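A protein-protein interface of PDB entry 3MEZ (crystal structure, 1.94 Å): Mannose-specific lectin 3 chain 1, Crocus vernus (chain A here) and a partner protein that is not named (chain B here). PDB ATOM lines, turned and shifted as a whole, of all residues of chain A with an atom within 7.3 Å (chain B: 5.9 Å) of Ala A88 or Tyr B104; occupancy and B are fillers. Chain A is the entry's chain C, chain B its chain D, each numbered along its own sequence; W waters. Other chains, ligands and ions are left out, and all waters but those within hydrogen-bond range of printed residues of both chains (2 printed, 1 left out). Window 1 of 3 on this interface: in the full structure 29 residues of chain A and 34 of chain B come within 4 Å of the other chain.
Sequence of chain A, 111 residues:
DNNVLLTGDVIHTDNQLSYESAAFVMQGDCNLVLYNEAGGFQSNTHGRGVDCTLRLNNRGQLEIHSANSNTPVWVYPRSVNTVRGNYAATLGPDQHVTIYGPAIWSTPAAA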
ATOM      1  N   VAL A   4     -21.398  22.630 -15.282  1.00  0.00           N
ATOM      2  CA  VAL A   4     -20.434  23.320 -16.121  1.00  0.00           C
ATOM      3  C   VAL A   4     -19.415  24.208 -15.372  1.00  0.00           C
ATOM      4  O   VAL A   4     -19.773  24.913 -14.508  1.00  0.00           O
ATOM      5  CB  VAL A   4     -21.154  24.142 -17.225  1.00  0.00           C
ATOM      6  CG1 VAL A   4     -20.195  24.926 -18.038  1.00  0.00           C
ATOM      7  CG2 VAL A   4     -21.952  23.259 -18.066  1.00  0.00           C
ATOM      8  N   LEU A   5     -18.145  24.137 -15.742  1.00  0.00           N
ATOM      9  CA  LEU A   5     -17.114  25.056 -15.292  1.00  0.00           C
ATOM     10  C   LEU A   5     -16.435  25.642 -16.518  1.00  0.00           C
ATOM     11  O   LEU A   5     -15.864  24.905 -17.247  1.00  0.00           O
ATOM     12  CB  LEU A   5     -16.049  24.323 -14.496  1.00  0.00           C
ATOM     13  CG  LEU A   5     -15.233  24.839 -13.305  1.00  0.00           C
ATOM     14  CD1 LEU A   5     -13.815  24.350 -13.284  1.00  0.00           C
ATOM     15  CD2 LEU A   5     -15.356  26.276 -12.988  1.00  0.00           C
ATOM     16  N   LEU A   6     -16.531  26.949 -16.684  1.00  0.00           N
ATOM     17  CA  LEU A   6     -15.850  27.703 -17.720  1.00  0.00           C
ATOM     18  C   LEU A   6     -14.511  28.288 -17.301  1.00  0.00           C
ATOM     19  O   LEU A   6     -14.307  28.535 -16.188  1.00  0.00           O
ATOM     20  CB  LEU A   6     -16.737  28.807 -18.277  1.00  0.00           C
ATOM     21  CG  LEU A   6     -18.193  28.487 -18.609  1.00  0.00           C
ATOM     22  CD1 LEU A   6     -18.870  29.688 -19.078  1.00  0.00           C
ATOM     23  CD2 LEU A   6     -18.323  27.364 -19.566  1.00  0.00           C
ATOM     24  N   THR A   7     -13.687  28.609 -18.279  1.00  0.00           N
ATOM     25  CA  THR A   7     -12.373  29.158 -18.059  1.00  0.00           C
ATOM     26  C   THR A   7     -12.487  30.403 -17.195  1.00  0.00           C
ATOM     27  O   THR A   7     -13.278  31.242 -17.416  1.00  0.00           O
ATOM     28  CB  THR A   7     -11.719  29.550 -19.435  1.00  0.00           C
ATOM     29  OG1 THR A   7     -11.387  28.399 -20.186  1.00  0.00           O
ATOM     30  CG2 THR A   7     -10.548  30.428 -19.272  1.00  0.00           C
ATOM     31  N   LEU A  56     -10.360  26.220 -14.113  1.00  0.00           N
ATOM     32  CA  LEU A  56     -10.101  25.839 -15.472  1.00  0.00           C
ATOM     33  C   LEU A  56      -9.438  27.022 -16.169  1.00  0.00           C
ATOM     34  O   LEU A  56      -9.963  28.095 -16.189  1.00  0.00           O
ATOM     35  CB  LEU A  56     -11.387  25.487 -16.186  1.00  0.00           C
ATOM     36  CG  LEU A  56     -11.225  25.024 -17.617  1.00  0.00           C
ATOM     37  CD1 LEU A  56     -10.488  23.801 -17.620  1.00  0.00           C
ATOM     38  CD2 LEU A  56     -12.546  24.818 -18.254  1.00  0.00           C
ATOM     39  N   ASN A  57      -8.277  26.774 -16.759  1.00  0.00           N
ATOM     40  CA  ASN A  57      -7.501  27.826 -17.371  1.00  0.00           C
ATOM     41  C   ASN A  57      -7.820  28.102 -18.842  1.00  0.00           C
ATOM     42  O   ASN A  57      -8.674  27.495 -19.408  1.00  0.00           O
ATOM     43  CB  ASN A  57      -5.977  27.717 -17.076  1.00  0.00           C
ATOM     44  CG  ASN A  57      -5.264  26.616 -17.852  1.00  0.00           C
ATOM     45  OD1 ASN A  57      -4.148  26.272 -17.533  1.00  0.00           O
ATOM     46  ND2 ASN A  57      -5.876  26.115 -18.840  1.00  0.00           N
ATOM     47  N   GLY A  60      -7.387  24.870 -21.310  1.00  0.00           N
ATOM     48  CA  GLY A  60      -8.123  23.657 -21.050  1.00  0.00           C
ATOM     49  C   GLY A  60      -7.616  22.751 -19.929  1.00  0.00           C
ATOM     50  O   GLY A  60      -8.043  21.649 -19.793  1.00  0.00           O
ATOM     51  N   GLY A  85      -7.512  30.472 -25.156  1.00  0.00           N
ATOM     52  CA  GLY A  85      -8.901  30.723 -25.401  1.00  0.00           C
ATOM     53  C   GLY A  85      -9.841  30.347 -24.271  1.00  0.00           C
ATOM     54  O   GLY A  85      -9.430  30.115 -23.195  1.00  0.00           O
ATOM     55  N   ASN A  86     -11.109  30.292 -24.590  1.00  0.00           N
ATOM     56  CA  ASN A  86     -12.120  29.892 -23.645  1.00  0.00           C
ATOM     57  C   ASN A  86     -12.487  28.407 -23.766  1.00  0.00           C
ATOM     58  O   ASN A  86     -12.803  27.951 -24.795  1.00  0.00           O
ATOM     59  CB  ASN A  86     -13.331  30.790 -23.774  1.00  0.00           C
ATOM     60  CG  ASN A  86     -13.033  32.224 -23.380  1.00  0.00           C
ATOM     61  OD1 ASN A  86     -12.101  32.480 -22.707  1.00  0.00           O
ATOM     62  ND2 ASN A  86     -13.843  33.127 -23.816  1.00  0.00           N
ATOM     63  N   TYR A  87     -12.466  27.722 -22.652  1.00  0.00           N
ATOM     64  CA  TYR A  87     -12.717  26.296 -22.545  1.00  0.00           C
ATOM     65  C   TYR A  87     -13.932  26.025 -21.577  1.00  0.00           C
ATOM     66  O   TYR A  87     -14.312  26.887 -20.842  1.00  0.00           O
ATOM     67  CB  TYR A  87     -11.434  25.576 -22.105  1.00  0.00           C
ATOM     68  CG  TYR A  87     -10.360  25.563 -23.192  1.00  0.00           C
ATOM     69  CD1 TYR A  87      -9.609  26.671 -23.455  1.00  0.00           C
ATOM     70  CD2 TYR A  87     -10.183  24.474 -23.994  1.00  0.00           C
ATOM     71  CE1 TYR A  87      -8.685  26.678 -24.463  1.00  0.00           C
ATOM     72  CE2 TYR A  87      -9.295  24.479 -24.994  1.00  0.00           C
ATOM     73  CZ  TYR A  87      -8.555  25.582 -25.242  1.00  0.00           C
ATOM     74  OH  TYR A  87      -7.680  25.533 -26.228  1.00  0.00           O
ATOM     75  N   ALA A  88     -14.524  24.850 -21.660  1.00  0.00           N
ATOM     76  CA  ALA A  88     -15.588  24.439 -20.772  1.00  0.00           C
ATOM     77  C   ALA A  88     -15.412  23.019 -20.285  1.00  0.00           C
ATOM     78  O   ALA A  88     -15.237  22.167 -21.092  1.00  0.00           O
ATOM     79  CB  ALA A  88     -16.851  24.567 -21.424  1.00  0.00           C
ATOM     80  N   ALA A  89     -15.500  22.809 -18.981  1.00  0.00           N
ATOM     81  CA  ALA A  89     -15.607  21.490 -18.400  1.00  0.00           C
ATOM     82  C   ALA A  89     -17.061  21.171 -18.137  1.00  0.00           C
ATOM     83  O   ALA A  89     -17.722  21.882 -17.462  1.00  0.00           O
ATOM     84  CB  ALA A  89     -14.827  21.367 -17.149  1.00  0.00           C
ATOM     85  N   THR A  90     -17.512  20.077 -18.697  1.00  0.00           N
ATOM     86  CA  THR A  90     -18.858  19.592 -18.532  1.00  0.00           C
ATOM     87  C   THR A  90     -18.915  18.181 -17.889  1.00  0.00           C
ATOM     88  O   THR A  90     -18.299  17.267 -18.367  1.00  0.00           O
ATOM     89  CB  THR A  90     -19.588  19.516 -19.894  1.00  0.00           C
ATOM     90  OG1 THR A  90     -19.576  20.773 -20.535  1.00  0.00           O
ATOM     91  CG2 THR A  90     -20.993  19.088 -19.717  1.00  0.00           C
ATOM     92  N   VAL A  97     -16.244  13.994 -16.550  1.00  0.00           N
ATOM     93  CA  VAL A  97     -15.931  15.359 -16.826  1.00  0.00           C
ATOM     94  C   VAL A  97     -15.071  15.419 -18.071  1.00  0.00           C
ATOM     95  O   VAL A  97     -14.013  14.871 -18.100  1.00  0.00           O
ATOM     96  CB  VAL A  97     -15.154  16.055 -15.685  1.00  0.00           C
ATOM     97  CG1 VAL A  97     -14.779  17.439 -16.096  1.00  0.00           C
ATOM     98  CG2 VAL A  97     -15.894  16.040 -14.396  1.00  0.00           C
ATOM     99  N   THR A  98     -15.570  16.101 -19.077  1.00  0.00           N
ATOM    100  CA  THR A  98     -14.860  16.302 -20.310  1.00  0.00           C
ATOM    101  C   THR A  98     -14.601  17.783 -20.549  1.00  0.00           C
ATOM    102  O   THR A  98     -15.477  18.580 -20.386  1.00  0.00           O
ATOM    103  CB  THR A  98     -15.578  15.705 -21.513  1.00  0.00           C
ATOM    104  OG1 THR A  98     -15.750  14.321 -21.332  1.00  0.00           O
ATOM    105  CG2 THR A  98     -14.760  15.923 -22.751  1.00  0.00           C
ATOM    106  N   ILE A  99     -13.374  18.116 -20.911  1.00  0.00           N
ATOM    107  CA  ILE A  99     -13.006  19.481 -21.205  1.00  0.00           C
ATOM    108  C   ILE A  99     -13.009  19.684 -22.720  1.00  0.00           C
ATOM    109  O   ILE A  99     -12.367  18.949 -23.430  1.00  0.00           O
ATOM    110  CB  ILE A  99     -11.626  19.868 -20.657  1.00  0.00           C
ATOM    111  CG1 ILE A  99     -11.681  20.109 -19.162  1.00  0.00           C
ATOM    112  CG2 ILE A  99     -11.147  21.114 -21.282  1.00  0.00           C
ATOM    113  CD1 ILE A  99     -12.326  19.135 -18.450  1.00  0.00           C
ATOM    114  N   TYR A 100     -13.740  20.694 -23.152  1.00  0.00           N
ATOM    115  CA  TYR A 100     -13.985  21.054 -24.541  1.00  0.00           C
ATOM    116  C   TYR A 100     -13.464  22.455 -24.878  1.00  0.00           C
ATOM    117  O   TYR A 100     -13.676  23.366 -24.158  1.00  0.00           O
ATOM    118  CB  TYR A 100     -15.480  21.032 -24.906  1.00  0.00           C
ATOM    119  CG  TYR A 100     -16.217  19.746 -24.725  1.00  0.00           C
ATOM    120  CD1 TYR A 100     -16.858  19.457 -23.544  1.00  0.00           C
ATOM    121  CD2 TYR A 100     -16.292  18.822 -25.737  1.00  0.00           C
ATOM    122  CE1 TYR A 100     -17.541  18.290 -23.382  1.00  0.00           C
ATOM    123  CE2 TYR A 100     -16.955  17.674 -25.574  1.00  0.00           C
ATOM    124  CZ  TYR A 100     -17.577  17.409 -24.400  1.00  0.00           C
ATOM    125  OH  TYR A 100     -18.237  16.287 -24.260  1.00  0.00           O
ATOM    126  N   GLY A 101     -12.804  22.602 -26.007  1.00  0.00           N
ATOM    127  CA  GLY A 101     -12.448  23.908 -26.491  1.00  0.00           C
ATOM    128  C   GLY A 101     -11.383  23.912 -27.561  1.00  0.00           C
ATOM    129  O   GLY A 101     -10.864  22.889 -27.903  1.00  0.00           O
ATOM    130  N   PRO A 102     -11.043  25.086 -28.044  1.00  0.00           N
ATOM    131  CA  PRO A 102     -11.573  26.349 -27.568  1.00  0.00           C
ATOM    132  C   PRO A 102     -12.951  26.699 -28.128  1.00  0.00           C
ATOM    133  O   PRO A 102     -13.459  26.018 -28.934  1.00  0.00           O
ATOM    134  CB  PRO A 102     -10.554  27.334 -28.090  1.00  0.00           C
ATOM    135  CG  PRO A 102     -10.146  26.774 -29.278  1.00  0.00           C
ATOM    136  CD  PRO A 102     -10.083  25.329 -29.113  1.00  0.00           C
ATOM    137  N   ALA A 103     -13.525  27.797 -27.691  1.00  0.00           N
ATOM    138  CA  ALA A 103     -14.783  28.222 -28.249  1.00  0.00           C
ATOM    139  C   ALA A 103     -14.639  28.500 -29.761  1.00  0.00           C
ATOM    140  O   ALA A 103     -13.727  29.120 -30.194  1.00  0.00           O
ATOM    141  CB  ALA A 103     -15.291  29.445 -27.551  1.00  0.00           C
ATOM    142  N   ILE A 104     -15.545  27.987 -30.546  1.00  0.00           N
ATOM    143  CA  ILE A 104     -15.478  28.250 -31.964  1.00  0.00           C
ATOM    144  C   ILE A 104     -16.565  29.081 -32.650  1.00  0.00           C
ATOM    145  O   ILE A 104     -16.346  29.569 -33.691  1.00  0.00           O
ATOM    146  CB  ILE A 104     -15.245  27.000 -32.742  1.00  0.00           C
ATOM    147  CG1 ILE A 104     -16.403  26.087 -32.589  1.00  0.00           C
ATOM    148  CG2 ILE A 104     -14.038  26.301 -32.224  1.00  0.00           C
ATOM    149  CD1 ILE A 104     -16.363  25.119 -33.543  1.00  0.00           C
ATOM    150  N   TRP A 105     -17.717  29.167 -32.033  1.00  0.00           N
ATOM    151  CA  TRP A 105     -18.814  29.986 -32.471  1.00  0.00           C
ATOM    152  C   TRP A 105     -19.618  30.399 -31.241  1.00  0.00           C
ATOM    153  O   TRP A 105     -19.760  29.646 -30.343  1.00  0.00           O
ATOM    154  CB  TRP A 105     -19.706  29.212 -33.425  1.00  0.00           C
ATOM    155  CG  TRP A 105     -20.925  29.907 -33.964  1.00  0.00           C
ATOM    156  CD1 TRP A 105     -21.021  30.577 -35.107  1.00  0.00           C
ATOM    157  CD2 TRP A 105     -22.210  29.950 -33.380  1.00  0.00           C
ATOM    158  NE1 TRP A 105     -22.261  31.039 -35.294  1.00  0.00           N
ATOM    159  CE2 TRP A 105     -23.019  30.678 -34.230  1.00  0.00           C
ATOM    160  CE3 TRP A 105     -22.744  29.478 -32.207  1.00  0.00           C
ATOM    161  CZ2 TRP A 105     -24.322  30.932 -33.947  1.00  0.00           C
ATOM    162  CZ3 TRP A 105     -24.032  29.725 -31.940  1.00  0.00           C
ATOM    163  CH2 TRP A 105     -24.810  30.433 -32.801  1.00  0.00           C
ATOM    164  N   SER A 106     -20.120  31.609 -31.259  1.00  0.00           N
ATOM    165  CA  SER A 106     -21.058  32.062 -30.283  1.00  0.00           C
ATOM    166  C   SER A 106     -21.994  33.147 -30.763  1.00  0.00           C
ATOM    167  O   SER A 106     -21.680  33.881 -31.656  1.00  0.00           O
ATOM    168  CB  SER A 106     -20.359  32.523 -29.034  1.00  0.00           C
ATOM    169  OG  SER A 106     -19.561  33.579 -29.319  1.00  0.00           O
ATOM    170  N   ASP B  90     -15.706  15.632 -30.737  1.00  0.00           N
ATOM    171  CA  ASP B  90     -16.922  15.852 -30.008  1.00  0.00           C
ATOM    172  C   ASP B  90     -16.975  17.287 -29.503  1.00  0.00           C
ATOM    173  O   ASP B  90     -16.031  17.777 -28.984  1.00  0.00           O
ATOM    174  CB  ASP B  90     -17.072  14.887 -28.847  1.00  0.00           C
ATOM    175  CG  ASP B  90     -17.072  13.420 -29.287  1.00  0.00           C
ATOM    176  OD1 ASP B  90     -17.429  13.140 -30.394  1.00  0.00           O
ATOM    177  OD2 ASP B  90     -16.740  12.590 -28.494  1.00  0.00           O
ATOM    178  N   TYR B  91     -18.113  17.901 -29.682  1.00  0.00           N
ATOM    179  CA  TYR B  91     -18.347  19.275 -29.339  1.00  0.00           C
ATOM    180  C   TYR B  91     -19.553  19.424 -28.416  1.00  0.00           C
ATOM    181  O   TYR B  91     -20.348  18.543 -28.270  1.00  0.00           O
ATOM    182  CB  TYR B  91     -18.537  20.120 -30.579  1.00  0.00           C
ATOM    183  CG  TYR B  91     -17.316  20.256 -31.459  1.00  0.00           C
ATOM    184  CD1 TYR B  91     -16.818  19.191 -32.163  1.00  0.00           C
ATOM    185  CD2 TYR B  91     -16.655  21.448 -31.563  1.00  0.00           C
ATOM    186  CE1 TYR B  91     -15.709  19.333 -32.973  1.00  0.00           C
ATOM    187  CE2 TYR B  91     -15.572  21.591 -32.323  1.00  0.00           C
ATOM    188  CZ  TYR B  91     -15.077  20.535 -33.035  1.00  0.00           C
ATOM    189  OH  TYR B  91     -13.981  20.690 -33.800  1.00  0.00           O
ATOM    190  N   VAL B  92     -19.631  20.587 -27.806  1.00  0.00           N
ATOM    191  CA  VAL B  92     -20.740  20.956 -27.012  1.00  0.00           C
ATOM    192  C   VAL B  92     -21.260  22.396 -27.316  1.00  0.00           C
ATOM    193  O   VAL B  92     -20.526  23.265 -27.568  1.00  0.00           O
ATOM    194  CB  VAL B  92     -20.393  20.749 -25.541  1.00  0.00           C
ATOM    195  CG1 VAL B  92     -19.623  21.837 -25.009  1.00  0.00           C
ATOM    196  CG2 VAL B  92     -21.557  20.520 -24.754  1.00  0.00           C
ATOM    197  N   LEU B  93     -22.566  22.542 -27.287  1.00  0.00           N
ATOM    198  CA  LEU B  93     -23.243  23.817 -27.296  1.00  0.00           C
ATOM    199  C   LEU B  93     -23.794  24.066 -25.902  1.00  0.00           C
ATOM    200  O   LEU B  93     -24.600  23.320 -25.422  1.00  0.00           O
ATOM    201  CB  LEU B  93     -24.405  23.732 -28.254  1.00  0.00           C
ATOM    202  CG  LEU B  93     -25.134  24.810 -29.008  1.00  0.00           C
ATOM    203  CD1 LEU B  93     -26.648  24.677 -28.983  1.00  0.00           C
ATOM    204  CD2 LEU B  93     -24.693  26.182 -28.739  1.00  0.00           C
ATOM    205  N   ILE B  94     -23.352  25.118 -25.279  1.00  0.00           N
ATOM    206  CA  ILE B  94     -23.827  25.496 -23.961  1.00  0.00           C
ATOM    207  C   ILE B  94     -24.607  26.822 -23.976  1.00  0.00           C
ATOM    208  O   ILE B  94     -24.140  27.785 -24.491  1.00  0.00           O
ATOM    209  CB  ILE B  94     -22.665  25.604 -22.946  1.00  0.00           C
ATOM    210  CG1 ILE B  94     -21.796  24.351 -22.953  1.00  0.00           C
ATOM    211  CG2 ILE B  94     -23.182  25.911 -21.558  1.00  0.00           C
ATOM    212  CD1 ILE B  94     -20.596  24.440 -22.193  1.00  0.00           C
ATOM    213  N   GLN B  96     -25.289  29.629 -21.854  1.00  0.00           N
ATOM    214  CA  GLN B  96     -24.642  30.191 -20.683  1.00  0.00           C
ATOM    215  C   GLN B  96     -25.442  31.159 -19.816  1.00  0.00           C
ATOM    216  O   GLN B  96     -26.357  31.768 -20.262  1.00  0.00           O
ATOM    217  CB  GLN B  96     -23.270  30.751 -21.022  1.00  0.00           C
ATOM    218  CG  GLN B  96     -22.384  29.804 -21.849  1.00  0.00           C
ATOM    219  CD  GLN B  96     -21.042  30.392 -22.160  1.00  0.00           C
ATOM    220  OE1 GLN B  96     -20.864  31.578 -22.093  1.00  0.00           O
ATOM    221  NE2 GLN B  96     -20.127  29.573 -22.494  1.00  0.00           N
ATOM    222  N   VAL B 102     -22.817  29.144 -26.906  1.00  0.00           N
ATOM    223  CA  VAL B 102     -21.453  28.986 -27.315  1.00  0.00           C
ATOM    224  C   VAL B 102     -21.092  27.543 -27.674  1.00  0.00           C
ATOM    225  O   VAL B 102     -21.399  26.653 -26.952  1.00  0.00           O
ATOM    226  CB  VAL B 102     -20.476  29.461 -26.230  1.00  0.00           C
ATOM    227  CG1 VAL B 102     -19.098  29.327 -26.659  1.00  0.00           C
ATOM    228  CG2 VAL B 102     -20.772  30.860 -25.777  1.00  0.00           C
ATOM    229  N   VAL B 103     -20.431  27.340 -28.785  1.00  0.00           N
ATOM    230  CA  VAL B 103     -19.949  26.009 -29.037  1.00  0.00           C
ATOM    231  C   VAL B 103     -18.470  25.874 -28.756  1.00  0.00           C
ATOM    232  O   VAL B 103     -17.684  26.676 -29.160  1.00  0.00           O
ATOM    233  CB  VAL B 103     -20.413  25.319 -30.357  1.00  0.00           C
ATOM    234  CG1 VAL B 103     -21.500  26.034 -31.095  1.00  0.00           C
ATOM    235  CG2 VAL B 103     -19.319  24.892 -31.168  1.00  0.00           C
ATOM    236  N   TYR B 104     -18.166  24.839 -28.007  1.00  0.00           N
ATOM    237  CA  TYR B 104     -16.849  24.508 -27.564  1.00  0.00           C
ATOM    238  C   TYR B 104     -16.436  23.126 -28.090  1.00  0.00           C
ATOM    239  O   TYR B 104     -17.153  22.203 -27.989  1.00  0.00           O
ATOM    240  CB  TYR B 104     -16.763  24.475 -26.037  1.00  0.00           C
ATOM    241  CG  TYR B 104     -16.962  25.760 -25.277  1.00  0.00           C
ATOM    242  CD1 TYR B 104     -18.196  26.108 -24.802  1.00  0.00           C
ATOM    243  CD2 TYR B 104     -15.913  26.618 -25.025  1.00  0.00           C
ATOM    244  CE1 TYR B 104     -18.400  27.272 -24.112  1.00  0.00           C
ATOM    245  CE2 TYR B 104     -16.103  27.776 -24.308  1.00  0.00           C
ATOM    246  CZ  TYR B 104     -17.356  28.114 -23.851  1.00  0.00           C
ATOM    247  OH  TYR B 104     -17.545  29.257 -23.173  1.00  0.00           O
ATOM    248  N   GLY B 105     -15.259  23.052 -28.653  1.00  0.00           N
ATOM    249  CA  GLY B 105     -14.645  21.796 -29.002  1.00  0.00           C
ATOM    250  C   GLY B 105     -13.402  21.898 -29.836  1.00  0.00           C
ATOM    251  O   GLY B 105     -13.055  22.973 -30.189  1.00  0.00           O
ATOM    252  N   PRO B 106     -12.767  20.773 -30.129  1.00  0.00           N
ATOM    253  CA  PRO B 106     -13.221  19.447 -29.715  1.00  0.00           C
ATOM    254  C   PRO B 106     -12.835  19.086 -28.265  1.00  0.00           C
ATOM    255  O   PRO B 106     -12.349  19.913 -27.577  1.00  0.00           O
ATOM    256  CB  PRO B 106     -12.453  18.547 -30.658  1.00  0.00           C
ATOM    257  CG  PRO B 106     -11.219  19.220 -30.844  1.00  0.00           C
ATOM    258  CD  PRO B 106     -11.438  20.680 -30.730  1.00  0.00           C
HETATM  259  O   HOH W   1     -15.347  29.379 -21.404  1.00  0.00           O
HETATM  260  O   HOH W   2     -20.007  15.923 -27.143  1.00  0.00           O
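The backbone carbonyl oxygen (O) of Pro B106 is in hydrogen-bond range of the backbone NH (N) of Gly A101 (3.1 Å).
The backbone NH (N) of Gly B105 is in hydrogen-bond range of the backbone carbonyl oxygen (O) of Pro A102 (3.5 Å).
O of Val B103 sits at hydrogen-bond distance from N of Ile A104, 2.9 Å away.
The backbone NH of Val B103 lies within hydrogen-bond range of the backbone carbonyl oxygen of Trp A105, at 2.9 Å.
The backbone carbonyl oxygen (O) of Gly A101 sits close to the backbone carbonyl oxygen (O) of Gly B105 (3.2 Å).
Tyr B104 touches Asn A86 (CE2 to O, 3.3 Å).
Tyr B104 touches Tyr A87.
CD2 of Tyr A100 touches O of Asp B90, 3.4 Å away.
Val B92 touches Tyr A100.
O of Tyr B104 touches CB of Tyr A100, at 3.7 Å.
Ala A103 touches Val B102 (CB to CG1, 3.9 Å).
Ala A103 touches Val B103 (CA to O, 3.4 Å).
Tyr B104 touches Ala A103 (CE2 to CB, 3.7 Å).
Ile A104 touches Tyr B91 (CD1 to CE2, 3.8 Å).
CB of Ser A106 touches CG2 of Val B102, at 3.7 Å.
Water W1 lies within hydrogen-bond range of the backbone carbonyl oxygen of Tyr A87 (2.8 Å) and the side-chain hydroxyl of Tyr B104 (2.8 Å).
Water W2 bridges O of Tyr B91 (2.9 Å) and OH of Tyr A100 (3.4 Å).
The backbone NH (N) of Tyr A87 lies within hydrogen-bond range of the side-chain hydroxyl (OG1) of Thr A7 (2.8 Å).
N of Ala A103 lies within hydrogen-bond range of O of Asn A86 (3.0 Å).
The backbone carbonyl oxygen (O) of Ala A88 is in hydrogen-bond range of the backbone NH (N) of Tyr A100 (2.9 Å).
The backbone NH of Tyr B104 lies within hydrogen-bond range of the backbone carbonyl oxygen of Val B92 (2.9 Å).
The backbone NH of Ile B94 lies within hydrogen-bond range of the backbone carbonyl oxygen of Val B102, 3.0 Å away.
The side-chain hydroxyl (OH) of Tyr B104 lies within hydrogen-bond range of the side-chain amide nitrogen (NE2) of Gln B96, 2.7 Å away.
Ala A88 touches just these residues of chain B: Ile B94 (3.8 Å) and Tyr B104 (3.9 Å).
Of chain A, only Asn A86 (3.3 Å), Tyr A87 (3.9 Å), Ala A88 (3.9 Å), Tyr A100 (3.7 Å), Pro A102 (3.96 Å) and Ala A103 (3.7 Å) come within 4 Å of Tyr B104.
Printed residues of chain B within 4 Å of Tyr A87: Tyr B104 (3.9 Å).
Of the printed residues of chain A, Pro B106 touches Tyr A100 (3.6 Å) and Gly A101 (3.1 Å).
Printed residues of chain B within 4 Å of Pro A102: Tyr B104 and Gly B105.
The nearest residue of chain B that does not touch Ala A88 is Val B92 (5.3 Å).
The nearest printed residue of chain A that does not touch Gln B96 is Ala A88 (6.1 Å).
Of the 23 printed residues of chain A, 11 touch a printed residue of chain B.
Printed residues of chain A that touch a printed residue of chain B: Leu A6, Asn A86, Tyr A87, Ala A88, Tyr A100, Gly A101, Pro A102, Ala A103, Ile A104, Trp A105 and Ser A106.
Along chain A the printed residues that touch a printed residue of chain B span positions 6 to 106.
Of the 11 printed residues of chain B, 10 touch a printed residue of chain A.
Hydrophobic or aromatic side chains of chain B within 4 Å of the printed part of chain A: Tyr B91, Val B92, Ile B94, Val B102, Val B103, Tyr B104 and Pro B106.
Among the printed residues, 21 pairs touch across the chains.
Among the printed residues, no Asp or Glu carboxylate lies within 4 Å of a Lys or Arg side-chain nitrogen of the other chain.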
